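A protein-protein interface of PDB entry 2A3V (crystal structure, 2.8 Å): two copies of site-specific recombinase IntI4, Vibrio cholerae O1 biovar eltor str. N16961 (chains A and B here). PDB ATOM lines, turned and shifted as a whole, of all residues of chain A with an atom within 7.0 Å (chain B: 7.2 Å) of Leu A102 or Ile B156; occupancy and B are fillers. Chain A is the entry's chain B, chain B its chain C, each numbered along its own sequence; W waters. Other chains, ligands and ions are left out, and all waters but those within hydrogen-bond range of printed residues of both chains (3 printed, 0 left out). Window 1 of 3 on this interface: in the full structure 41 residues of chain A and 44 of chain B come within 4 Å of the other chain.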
ATOM      1  N   GLU A  99     -16.747   5.603 -14.864  1.00  0.00           N
ATOM      2  CA  GLU A  99     -15.410   5.698 -15.412  1.00  0.00           C
ATOM      3  C   GLU A  99     -15.066   4.532 -16.313  1.00  0.00           C
ATOM      4  O   GLU A  99     -14.662   3.476 -15.848  1.00  0.00           O
ATOM      5  CB  GLU A  99     -14.400   5.794 -14.271  1.00  0.00           C
ATOM      6  CG  GLU A  99     -13.137   6.538 -14.664  1.00  0.00           C
ATOM      7  CD  GLU A  99     -13.403   8.005 -14.988  1.00  0.00           C
ATOM      8  OE1 GLU A  99     -12.643   8.569 -15.819  1.00  0.00           O
ATOM      9  OE2 GLU A  99     -14.359   8.584 -14.401  1.00  0.00           O
ATOM     10  N   ARG A 100     -15.211   4.736 -17.613  1.00  0.00           N
ATOM     11  CA  ARG A 100     -14.927   3.679 -18.569  1.00  0.00           C
ATOM     12  C   ARG A 100     -13.430   3.409 -18.764  1.00  0.00           C
ATOM     13  O   ARG A 100     -12.573   4.225 -18.413  1.00  0.00           O
ATOM     14  CB  ARG A 100     -15.606   3.985 -19.914  1.00  0.00           C
ATOM     15  CG  ARG A 100     -17.148   4.111 -19.828  1.00  0.00           C
ATOM     16  CD  ARG A 100     -17.810   2.899 -19.130  1.00  0.00           C
ATOM     17  NE  ARG A 100     -19.203   3.144 -18.730  1.00  0.00           N
ATOM     18  CZ  ARG A 100     -19.711   2.830 -17.531  1.00  0.00           C
ATOM     19  NH1 ARG A 100     -18.941   2.259 -16.597  1.00  0.00           N
ATOM     20  NH2 ARG A 100     -20.992   3.079 -17.262  1.00  0.00           N
ATOM     21  N   LYS A 101     -13.130   2.236 -19.303  1.00  0.00           N
ATOM     22  CA  LYS A 101     -11.761   1.838 -19.539  1.00  0.00           C
ATOM     23  C   LYS A 101     -11.203   2.649 -20.657  1.00  0.00           C
ATOM     24  O   LYS A 101     -11.942   3.132 -21.501  1.00  0.00           O
ATOM     25  CB  LYS A 101     -11.698   0.368 -19.930  1.00  0.00           C
ATOM     26  CG  LYS A 101     -12.042  -0.596 -18.813  1.00  0.00           C
ATOM     27  CD  LYS A 101     -12.074  -2.024 -19.308  1.00  0.00           C
ATOM     28  CE  LYS A 101     -10.740  -2.447 -19.890  1.00  0.00           C
ATOM     29  NZ  LYS A 101     -10.753  -3.860 -20.364  1.00  0.00           N
ATOM     30  N   LEU A 102      -9.890   2.800 -20.662  1.00  0.00           N
ATOM     31  CA  LEU A 102      -9.244   3.536 -21.725  1.00  0.00           C
ATOM     32  C   LEU A 102      -9.084   2.559 -22.886  1.00  0.00           C
ATOM     33  O   LEU A 102      -8.362   1.572 -22.788  1.00  0.00           O
ATOM     34  CB  LEU A 102      -7.880   4.027 -21.273  1.00  0.00           C
ATOM     35  CG  LEU A 102      -7.906   5.039 -20.139  1.00  0.00           C
ATOM     36  CD1 LEU A 102      -6.470   5.321 -19.718  1.00  0.00           C
ATOM     37  CD2 LEU A 102      -8.598   6.306 -20.573  1.00  0.00           C
ATOM     38  N   PRO A 103      -9.765   2.819 -24.004  1.00  0.00           N
ATOM     39  CA  PRO A 103      -9.668   1.931 -25.159  1.00  0.00           C
ATOM     40  C   PRO A 103      -8.239   1.767 -25.643  1.00  0.00           C
ATOM     41  O   PRO A 103      -7.437   2.691 -25.550  1.00  0.00           O
ATOM     42  CB  PRO A 103     -10.541   2.625 -26.190  1.00  0.00           C
ATOM     43  CG  PRO A 103     -10.340   4.074 -25.856  1.00  0.00           C
ATOM     44  CD  PRO A 103     -10.486   4.053 -24.353  1.00  0.00           C
ATOM     45  N   VAL A 104      -7.940   0.575 -26.146  1.00  0.00           N
ATOM     46  CA  VAL A 104      -6.635   0.221 -26.690  1.00  0.00           C
ATOM     47  C   VAL A 104      -6.921  -0.350 -28.079  1.00  0.00           C
ATOM     48  O   VAL A 104      -7.576  -1.390 -28.197  1.00  0.00           O
ATOM     49  CB  VAL A 104      -5.954  -0.836 -25.792  1.00  0.00           C
ATOM     50  CG1 VAL A 104      -4.893  -1.608 -26.573  1.00  0.00           C
ATOM     51  CG2 VAL A 104      -5.316  -0.146 -24.585  1.00  0.00           C
ATOM     52  N   VAL A 105      -6.465   0.332 -29.127  1.00  0.00           N
ATOM     53  CA  VAL A 105      -6.724  -0.147 -30.486  1.00  0.00           C
ATOM     54  C   VAL A 105      -5.511  -0.751 -31.153  1.00  0.00           C
ATOM     55  O   VAL A 105      -4.380  -0.451 -30.793  1.00  0.00           O
ATOM     56  CB  VAL A 105      -7.238   0.961 -31.420  1.00  0.00           C
ATOM     57  CG1 VAL A 105      -8.403   1.688 -30.777  1.00  0.00           C
ATOM     58  CG2 VAL A 105      -6.113   1.898 -31.768  1.00  0.00           C
ATOM     59  N   HIS A 271     -13.081  -1.446 -30.722  1.00  0.00           N
ATOM     60  CA  HIS A 271     -12.469  -0.162 -30.481  1.00  0.00           C
ATOM     61  C   HIS A 271     -11.741   0.269 -31.722  1.00  0.00           C
ATOM     62  O   HIS A 271     -11.773   1.435 -32.116  1.00  0.00           O
ATOM     63  CB  HIS A 271     -11.453  -0.227 -29.338  1.00  0.00           C
ATOM     64  CG  HIS A 271     -12.042  -0.597 -28.011  1.00  0.00           C
ATOM     65  ND1 HIS A 271     -13.348  -0.314 -27.670  1.00  0.00           N
ATOM     66  CD2 HIS A 271     -11.493  -1.198 -26.930  1.00  0.00           C
ATOM     67  CE1 HIS A 271     -13.581  -0.726 -26.438  1.00  0.00           C
ATOM     68  NE2 HIS A 271     -12.472  -1.267 -25.964  1.00  0.00           N
ATOM     69  N   ILE A 301     -14.514   9.094 -26.387  1.00  0.00           N
ATOM     70  CA  ILE A 301     -13.314   8.517 -25.813  1.00  0.00           C
ATOM     71  C   ILE A 301     -12.356   8.062 -26.903  1.00  0.00           C
ATOM     72  O   ILE A 301     -11.145   8.186 -26.755  1.00  0.00           O
ATOM     73  CB  ILE A 301     -13.648   7.324 -24.946  1.00  0.00           C
ATOM     74  CG1 ILE A 301     -14.822   7.687 -24.016  1.00  0.00           C
ATOM     75  CG2 ILE A 301     -12.425   6.925 -24.133  1.00  0.00           C
ATOM     76  CD1 ILE A 301     -15.567   6.468 -23.369  1.00  0.00           C
ATOM     77  N   HIS A 304      -9.770  10.781 -27.990  1.00  0.00           N
ATOM     78  CA  HIS A 304      -8.647  11.166 -27.164  1.00  0.00           C
ATOM     79  C   HIS A 304      -7.275  10.737 -27.639  1.00  0.00           C
ATOM     80  O   HIS A 304      -6.405  11.564 -27.890  1.00  0.00           O
ATOM     81  CB  HIS A 304      -8.890  10.663 -25.755  1.00  0.00           C
ATOM     82  CG  HIS A 304     -10.171  11.155 -25.161  1.00  0.00           C
ATOM     83  ND1 HIS A 304     -10.643  10.720 -23.942  1.00  0.00           N
ATOM     84  CD2 HIS A 304     -11.082  12.048 -25.619  1.00  0.00           C
ATOM     85  CE1 HIS A 304     -11.789  11.322 -23.674  1.00  0.00           C
ATOM     86  NE2 HIS A 304     -12.077  12.134 -24.675  1.00  0.00           N
ATOM     87  N   SER B 132       4.511  15.244 -19.924  1.00  0.00           N
ATOM     88  CA  SER B 132       3.132  14.801 -19.963  1.00  0.00           C
ATOM     89  C   SER B 132       2.413  15.202 -18.693  1.00  0.00           C
ATOM     90  O   SER B 132       1.397  14.610 -18.329  1.00  0.00           O
ATOM     91  CB  SER B 132       3.074  13.284 -20.117  1.00  0.00           C
ATOM     92  OG  SER B 132       3.915  12.841 -21.167  1.00  0.00           O
ATOM     93  N   LEU B 134       2.549  14.461 -15.725  1.00  0.00           N
ATOM     94  CA  LEU B 134       2.105  13.407 -14.817  1.00  0.00           C
ATOM     95  C   LEU B 134       2.339  13.733 -13.357  1.00  0.00           C
ATOM     96  O   LEU B 134       3.222  14.516 -13.022  1.00  0.00           O
ATOM     97  CB  LEU B 134       2.826  12.091 -15.118  1.00  0.00           C
ATOM     98  CG  LEU B 134       2.634  11.549 -16.526  1.00  0.00           C
ATOM     99  CD1 LEU B 134       3.224  10.158 -16.605  1.00  0.00           C
ATOM    100  CD2 LEU B 134       1.140  11.526 -16.878  1.00  0.00           C
ATOM    101  N   ARG B 135       1.547  13.125 -12.481  1.00  0.00           N
ATOM    102  CA  ARG B 135       1.743  13.301 -11.054  1.00  0.00           C
ATOM    103  C   ARG B 135       2.804  12.292 -10.692  1.00  0.00           C
ATOM    104  O   ARG B 135       3.059  11.359 -11.457  1.00  0.00           O
ATOM    105  CB  ARG B 135       0.472  13.020 -10.283  1.00  0.00           C
ATOM    106  CG  ARG B 135      -0.483  14.180 -10.309  1.00  0.00           C
ATOM    107  CD  ARG B 135      -1.645  13.984  -9.370  1.00  0.00           C
ATOM    108  NE  ARG B 135      -2.774  13.509 -10.140  1.00  0.00           N
ATOM    109  CZ  ARG B 135      -3.879  14.211 -10.383  1.00  0.00           C
ATOM    110  NH1 ARG B 135      -4.030  15.439  -9.897  1.00  0.00           N
ATOM    111  NH2 ARG B 135      -4.819  13.684 -11.161  1.00  0.00           N
ATOM    112  N   GLU B 138       1.575   8.787 -10.501  1.00  0.00           N
ATOM    113  CA  GLU B 138       1.052   8.365 -11.808  1.00  0.00           C
ATOM    114  C   GLU B 138       2.198   7.857 -12.648  1.00  0.00           C
ATOM    115  O   GLU B 138       2.090   6.830 -13.309  1.00  0.00           O
ATOM    116  CB  GLU B 138       0.355   9.512 -12.556  1.00  0.00           C
ATOM    117  CG  GLU B 138      -0.998   9.895 -11.977  1.00  0.00           C
ATOM    118  CD  GLU B 138      -1.623  11.111 -12.640  1.00  0.00           C
ATOM    119  OE1 GLU B 138      -0.929  11.833 -13.388  1.00  0.00           O
ATOM    120  OE2 GLU B 138      -2.820  11.353 -12.390  1.00  0.00           O
ATOM    121  N   CYS B 139       3.310   8.579 -12.610  1.00  0.00           N
ATOM    122  CA  CYS B 139       4.481   8.190 -13.385  1.00  0.00           C
ATOM    123  C   CYS B 139       5.106   6.899 -12.870  1.00  0.00           C
ATOM    124  O   CYS B 139       5.472   6.025 -13.652  1.00  0.00           O
ATOM    125  CB  CYS B 139       5.531   9.287 -13.338  1.00  0.00           C
ATOM    126  SG  CYS B 139       6.946   8.876 -14.349  1.00  0.00           S
ATOM    127  N   LEU B 142       3.170   3.609 -13.815  1.00  0.00           N
ATOM    128  CA  LEU B 142       3.004   3.253 -15.213  1.00  0.00           C
ATOM    129  C   LEU B 142       3.320   1.779 -15.493  1.00  0.00           C
ATOM    130  O   LEU B 142       4.090   1.158 -14.766  1.00  0.00           O
ATOM    131  CB  LEU B 142       3.888   4.147 -16.082  1.00  0.00           C
ATOM    132  CG  LEU B 142       3.421   5.587 -16.274  1.00  0.00           C
ATOM    133  CD1 LEU B 142       4.467   6.354 -17.068  1.00  0.00           C
ATOM    134  CD2 LEU B 142       2.091   5.608 -17.021  1.00  0.00           C
ATOM    135  N   ASP B 146       0.842   0.674 -20.883  1.00  0.00           N
ATOM    136  CA  ASP B 146       0.340   2.033 -20.780  1.00  0.00           C
ATOM    137  C   ASP B 146       0.969   3.028 -21.754  1.00  0.00           C
ATOM    138  O   ASP B 146       0.447   4.128 -21.953  1.00  0.00           O
ATOM    139  CB  ASP B 146       0.473   2.546 -19.338  1.00  0.00           C
ATOM    140  CG  ASP B 146      -0.331   1.717 -18.323  1.00  0.00           C
ATOM    141  OD1 ASP B 146      -1.213   0.930 -18.727  1.00  0.00           O
ATOM    142  OD2 ASP B 146      -0.082   1.863 -17.102  1.00  0.00           O
ATOM    143  N   ILE B 154      -0.038   8.469 -23.553  1.00  0.00           N
ATOM    144  CA  ILE B 154       0.149   7.619 -22.394  1.00  0.00           C
ATOM    145  C   ILE B 154      -1.195   7.450 -21.714  1.00  0.00           C
ATOM    146  O   ILE B 154      -1.930   8.428 -21.504  1.00  0.00           O
ATOM    147  CB  ILE B 154       1.093   8.222 -21.350  1.00  0.00           C
ATOM    148  CG1 ILE B 154       2.439   8.533 -21.961  1.00  0.00           C
ATOM    149  CG2 ILE B 154       1.291   7.231 -20.211  1.00  0.00           C
ATOM    150  CD1 ILE B 154       3.368   9.198 -20.971  1.00  0.00           C
ATOM    151  N   ARG B 155      -1.518   6.207 -21.371  1.00  0.00           N
ATOM    152  CA  ARG B 155      -2.775   5.925 -20.702  1.00  0.00           C
ATOM    153  C   ARG B 155      -2.545   5.977 -19.203  1.00  0.00           C
ATOM    154  O   ARG B 155      -1.818   5.162 -18.662  1.00  0.00           O
ATOM    155  CB  ARG B 155      -3.293   4.545 -21.109  1.00  0.00           C
ATOM    156  CG  ARG B 155      -4.125   4.533 -22.383  1.00  0.00           C
ATOM    157  CD  ARG B 155      -4.436   3.099 -22.787  1.00  0.00           C
ATOM    158  NE  ARG B 155      -3.231   2.476 -23.307  1.00  0.00           N
ATOM    159  CZ  ARG B 155      -2.824   2.611 -24.560  1.00  0.00           C
ATOM    160  NH1 ARG B 155      -3.547   3.330 -25.418  1.00  0.00           N
ATOM    161  NH2 ARG B 155      -1.665   2.082 -24.937  1.00  0.00           N
ATOM    162  N   ILE B 156      -3.143   6.948 -18.529  1.00  0.00           N
ATOM    163  CA  ILE B 156      -2.976   7.055 -17.089  1.00  0.00           C
ATOM    164  C   ILE B 156      -4.196   6.423 -16.463  1.00  0.00           C
ATOM    165  O   ILE B 156      -5.290   7.009 -16.451  1.00  0.00           O
ATOM    166  CB  ILE B 156      -2.887   8.523 -16.639  1.00  0.00           C
ATOM    167  CG1 ILE B 156      -1.729   9.222 -17.346  1.00  0.00           C
ATOM    168  CG2 ILE B 156      -2.665   8.591 -15.175  1.00  0.00           C
ATOM    169  CD1 ILE B 156      -0.432   8.456 -17.275  1.00  0.00           C
ATOM    170  N   TRP B 157      -4.026   5.214 -15.953  1.00  0.00           N
ATOM    171  CA  TRP B 157      -5.152   4.518 -15.364  1.00  0.00           C
ATOM    172  C   TRP B 157      -5.416   4.898 -13.928  1.00  0.00           C
ATOM    173  O   TRP B 157      -4.488   5.030 -13.129  1.00  0.00           O
ATOM    174  CB  TRP B 157      -4.942   3.013 -15.447  1.00  0.00           C
ATOM    175  CG  TRP B 157      -5.095   2.456 -16.818  1.00  0.00           C
ATOM    176  CD1 TRP B 157      -4.133   2.364 -17.778  1.00  0.00           C
ATOM    177  CD2 TRP B 157      -6.282   1.887 -17.384  1.00  0.00           C
ATOM    178  NE1 TRP B 157      -4.639   1.764 -18.911  1.00  0.00           N
ATOM    179  CE2 TRP B 157      -5.960   1.465 -18.697  1.00  0.00           C
ATOM    180  CE3 TRP B 157      -7.587   1.693 -16.913  1.00  0.00           C
ATOM    181  CZ2 TRP B 157      -6.903   0.857 -19.545  1.00  0.00           C
ATOM    182  CZ3 TRP B 157      -8.522   1.086 -17.757  1.00  0.00           C
ATOM    183  CH2 TRP B 157      -8.171   0.677 -19.057  1.00  0.00           C
ATOM    184  N   GLN B 158      -6.684   5.100 -13.603  1.00  0.00           N
ATOM    185  CA  GLN B 158      -7.055   5.418 -12.238  1.00  0.00           C
ATOM    186  C   GLN B 158      -6.216   6.496 -11.542  1.00  0.00           C
ATOM    187  O   GLN B 158      -5.613   6.240 -10.508  1.00  0.00           O
ATOM    188  CB  GLN B 158      -6.986   4.142 -11.418  1.00  0.00           C
ATOM    189  CG  GLN B 158      -8.065   3.142 -11.730  1.00  0.00           C
ATOM    190  CD  GLN B 158      -9.431   3.691 -11.411  1.00  0.00           C
ATOM    191  OE1 GLN B 158      -9.936   3.531 -10.288  1.00  0.00           O
ATOM    192  NE2 GLN B 158     -10.059   4.329 -12.402  1.00  0.00           N
ATOM    193  N   GLY B 159      -6.163   7.700 -12.098  1.00  0.00           N
ATOM    194  CA  GLY B 159      -5.400   8.766 -11.464  1.00  0.00           C
ATOM    195  C   GLY B 159      -6.186   9.276 -10.268  1.00  0.00           C
ATOM    196  O   GLY B 159      -7.196   8.676  -9.900  1.00  0.00           O
ATOM    197  N   LYS B 160      -5.763  10.379  -9.660  1.00  0.00           N
ATOM    198  CA  LYS B 160      -6.481  10.878  -8.492  1.00  0.00           C
ATOM    199  C   LYS B 160      -7.985  10.778  -8.631  1.00  0.00           C
ATOM    200  O   LYS B 160      -8.558  11.214  -9.620  1.00  0.00           O
ATOM    201  CB  LYS B 160      -6.113  12.327  -8.199  1.00  0.00           C
ATOM    202  CG  LYS B 160      -6.704  12.843  -6.893  1.00  0.00           C
ATOM    203  CD  LYS B 160      -6.133  14.204  -6.560  1.00  0.00           C
ATOM    204  CE  LYS B 160      -6.798  14.839  -5.349  1.00  0.00           C
ATOM    205  NZ  LYS B 160      -6.147  16.154  -5.063  1.00  0.00           N
ATOM    206  N   LYS B 163     -10.031   8.196 -11.825  1.00  0.00           N
ATOM    207  CA  LYS B 163     -10.401   8.737 -13.130  1.00  0.00           C
ATOM    208  C   LYS B 163      -9.349   8.346 -14.134  1.00  0.00           C
ATOM    209  O   LYS B 163      -8.162   8.411 -13.847  1.00  0.00           O
ATOM    210  CB  LYS B 163     -10.523  10.257 -13.054  1.00  0.00           C
ATOM    211  CG  LYS B 163     -11.889  10.714 -12.534  1.00  0.00           C
ATOM    212  CD  LYS B 163     -11.842  12.070 -11.806  1.00  0.00           C
ATOM    213  CE  LYS B 163     -11.086  13.168 -12.588  1.00  0.00           C
ATOM    214  NZ  LYS B 163     -11.656  13.512 -13.941  1.00  0.00           N
ATOM    215  N   ASN B 164      -9.772   7.919 -15.312  1.00  0.00           N
ATOM    216  CA  ASN B 164      -8.794   7.526 -16.302  1.00  0.00           C
ATOM    217  C   ASN B 164      -8.641   8.646 -17.282  1.00  0.00           C
ATOM    218  O   ASN B 164      -9.571   9.408 -17.482  1.00  0.00           O
ATOM    219  CB  ASN B 164      -9.246   6.266 -17.025  1.00  0.00           C
ATOM    220  CG  ASN B 164      -9.542   5.136 -16.081  1.00  0.00           C
ATOM    221  OD1 ASN B 164      -8.728   4.801 -15.229  1.00  0.00           O
ATOM    222  ND2 ASN B 164     -10.710   4.540 -16.226  1.00  0.00           N
ATOM    223  N   ARG B 165      -7.461   8.779 -17.871  1.00  0.00           N
ATOM    224  CA  ARG B 165      -7.271   9.815 -18.861  1.00  0.00           C
ATOM    225  C   ARG B 165      -6.152   9.450 -19.806  1.00  0.00           C
ATOM    226  O   ARG B 165      -5.360   8.551 -19.520  1.00  0.00           O
ATOM    227  CB  ARG B 165      -7.025  11.177 -18.207  1.00  0.00           C
ATOM    228  CG  ARG B 165      -5.687  11.411 -17.534  1.00  0.00           C
ATOM    229  CD  ARG B 165      -5.633  12.836 -16.935  1.00  0.00           C
ATOM    230  NE  ARG B 165      -4.264  13.264 -16.672  1.00  0.00           N
ATOM    231  CZ  ARG B 165      -3.570  12.925 -15.598  1.00  0.00           C
ATOM    232  NH1 ARG B 165      -4.123  12.167 -14.662  1.00  0.00           N
ATOM    233  NH2 ARG B 165      -2.305  13.303 -15.488  1.00  0.00           N
ATOM    234  N   THR B 166      -6.117  10.126 -20.950  1.00  0.00           N
ATOM    235  CA  THR B 166      -5.108   9.880 -21.971  1.00  0.00           C
ATOM    236  C   THR B 166      -4.339  11.155 -22.132  1.00  0.00           C
ATOM    237  O   THR B 166      -4.889  12.182 -22.511  1.00  0.00           O
ATOM    238  CB  THR B 166      -5.725   9.563 -23.311  1.00  0.00           C
ATOM    239  OG1 THR B 166      -6.819   8.670 -23.115  1.00  0.00           O
ATOM    240  CG2 THR B 166      -4.714   8.903 -24.199  1.00  0.00           C
ATOM    241  N   VAL B 167      -3.052  11.089 -21.887  1.00  0.00           N
ATOM    242  CA  VAL B 167      -2.255  12.283 -21.953  1.00  0.00           C
ATOM    243  C   VAL B 167      -1.317  12.254 -23.150  1.00  0.00           C
ATOM    244  O   VAL B 167      -1.103  11.200 -23.732  1.00  0.00           O
ATOM    245  CB  VAL B 167      -1.487  12.391 -20.634  1.00  0.00           C
ATOM    246  CG1 VAL B 167      -0.242  11.531 -20.703  1.00  0.00           C
ATOM    247  CG2 VAL B 167      -1.189  13.807 -20.329  1.00  0.00           C
ATOM    248  N   GLN B 290      -5.687  17.388 -20.254  1.00  0.00           N
ATOM    249  CA  GLN B 290      -4.390  16.756 -20.031  1.00  0.00           C
ATOM    250  C   GLN B 290      -4.151  16.560 -18.531  1.00  0.00           C
ATOM    251  O   GLN B 290      -3.575  15.569 -18.128  1.00  0.00           O
ATOM    252  CB  GLN B 290      -3.264  17.612 -20.617  1.00  0.00           C
ATOM    253  CG  GLN B 290      -3.282  17.731 -22.129  1.00  0.00           C
ATOM    254  CD  GLN B 290      -2.876  16.450 -22.842  1.00  0.00           C
ATOM    255  OE1 GLN B 290      -3.538  16.033 -23.795  1.00  0.00           O
ATOM    256  NE2 GLN B 290      -1.784  15.828 -22.398  1.00  0.00           N
HETATM  257  O   HOH W   1      -9.042   9.863 -21.821  1.00  0.00           O
HETATM  258  O   HOH W   2      -5.867   4.761 -25.635  1.00  0.00           O
HETATM  259  O   HOH W   3     -11.840  11.122 -16.705  1.00  0.00           O
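ND2 of Asn B164 lies within hydrogen-bond range of O of Arg A100, 2.9 Å away.
The backbone NH (N) of Asn B164 lies within hydrogen-bond range of the side-chain carboxylate (OE1) of Glu A99 (3.0 Å).
NE of Arg B165 lies within hydrogen-bond range of O of Gln B290, 2.8 Å away.
The backbone carbonyl oxygen (O) of Asp B146 lies within hydrogen-bond range of the backbone NH (N) of Arg B155 (2.9 Å).
OD1 of Asn B164 sits at hydrogen-bond distance from N of Gln B158, at 2.6 Å.
NH1 of Arg B165 lies within salt-bridge range of OE2 of Glu B138, 2.7 Å away.
The backbone NH of Ile B156 is in hydrogen-bond range of the backbone carbonyl oxygen of Arg B165 (2.9 Å).
Glu A99 touches Lys B163 (OE1 to CA, 3.5 Å).
Lys A101 touches Trp B157.
CD1 of Leu A102 touches CB of Arg B155 (3.6 Å).
Trp B157 touches Leu A102 (CH2 to N, 3.2 Å).
Asn B164 touches Leu A102.
Leu A102 touches Arg B165.
OG1 of Thr B166 touches CD2 of Leu A102 (3.9 Å).
NH1 of Arg B155 touches O of Pro A103 (3.9 Å).
Arg B155 touches Val A104 (NE to CG2, 3.6 Å).
CB of His A304 touches OG1 of Thr B166, at 3.9 Å.
Of the printed residues of chain B, Leu A102 touches Arg B155, Ile B156, Trp B157, Asn B164, Arg B165 and Thr B166.
Of chain A, only Leu A102 comes within 4 Å of Ile B156.
Of the printed residues of chain B, Val A104 touches Arg B155 (3.6 Å).
Printed residues of chain B within 4 Å of His A304: Thr B166 (3.9 Å).
Of the printed residues of chain A, Trp B157 touches Lys A101 (3.6 Å) and Leu A102 (3.2 Å).
Of the 20 printed residues of chain B, 7 touch a printed residue of chain A.
Printed residues of chain B that touch a printed residue of chain A: Arg B155, Ile B156, Trp B157, Lys B163, Asn B164, Arg B165 and Thr B166.
Hydrophobic or aromatic side chains of chain B that line the printed part of chain A: Trp B157.
Of the 10 printed residues of chain A, 7 touch a printed residue of chain B.
Hydrophobic or aromatic side chains of chain A within 4 Å of the printed part of chain B: Leu A102, Val A104 and His A304.
Among the printed residues, 13 pairs touch across the chains.
No position is printed for both chains.
Water W2 bridges the backbone carbonyl oxygen of Pro A103 (2.6 Å) and the guanidinium group of Arg B155 (2.7 Å).
Water W1 lies within hydrogen-bond range of ND1 of His A304 (2.8 Å) and OG1 of Thr B166 (2.8 Å).
Water W3 lies within hydrogen-bond range of OE1 of Glu A99 (2.8 Å) and O of Asn B164 (2.9 Å).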
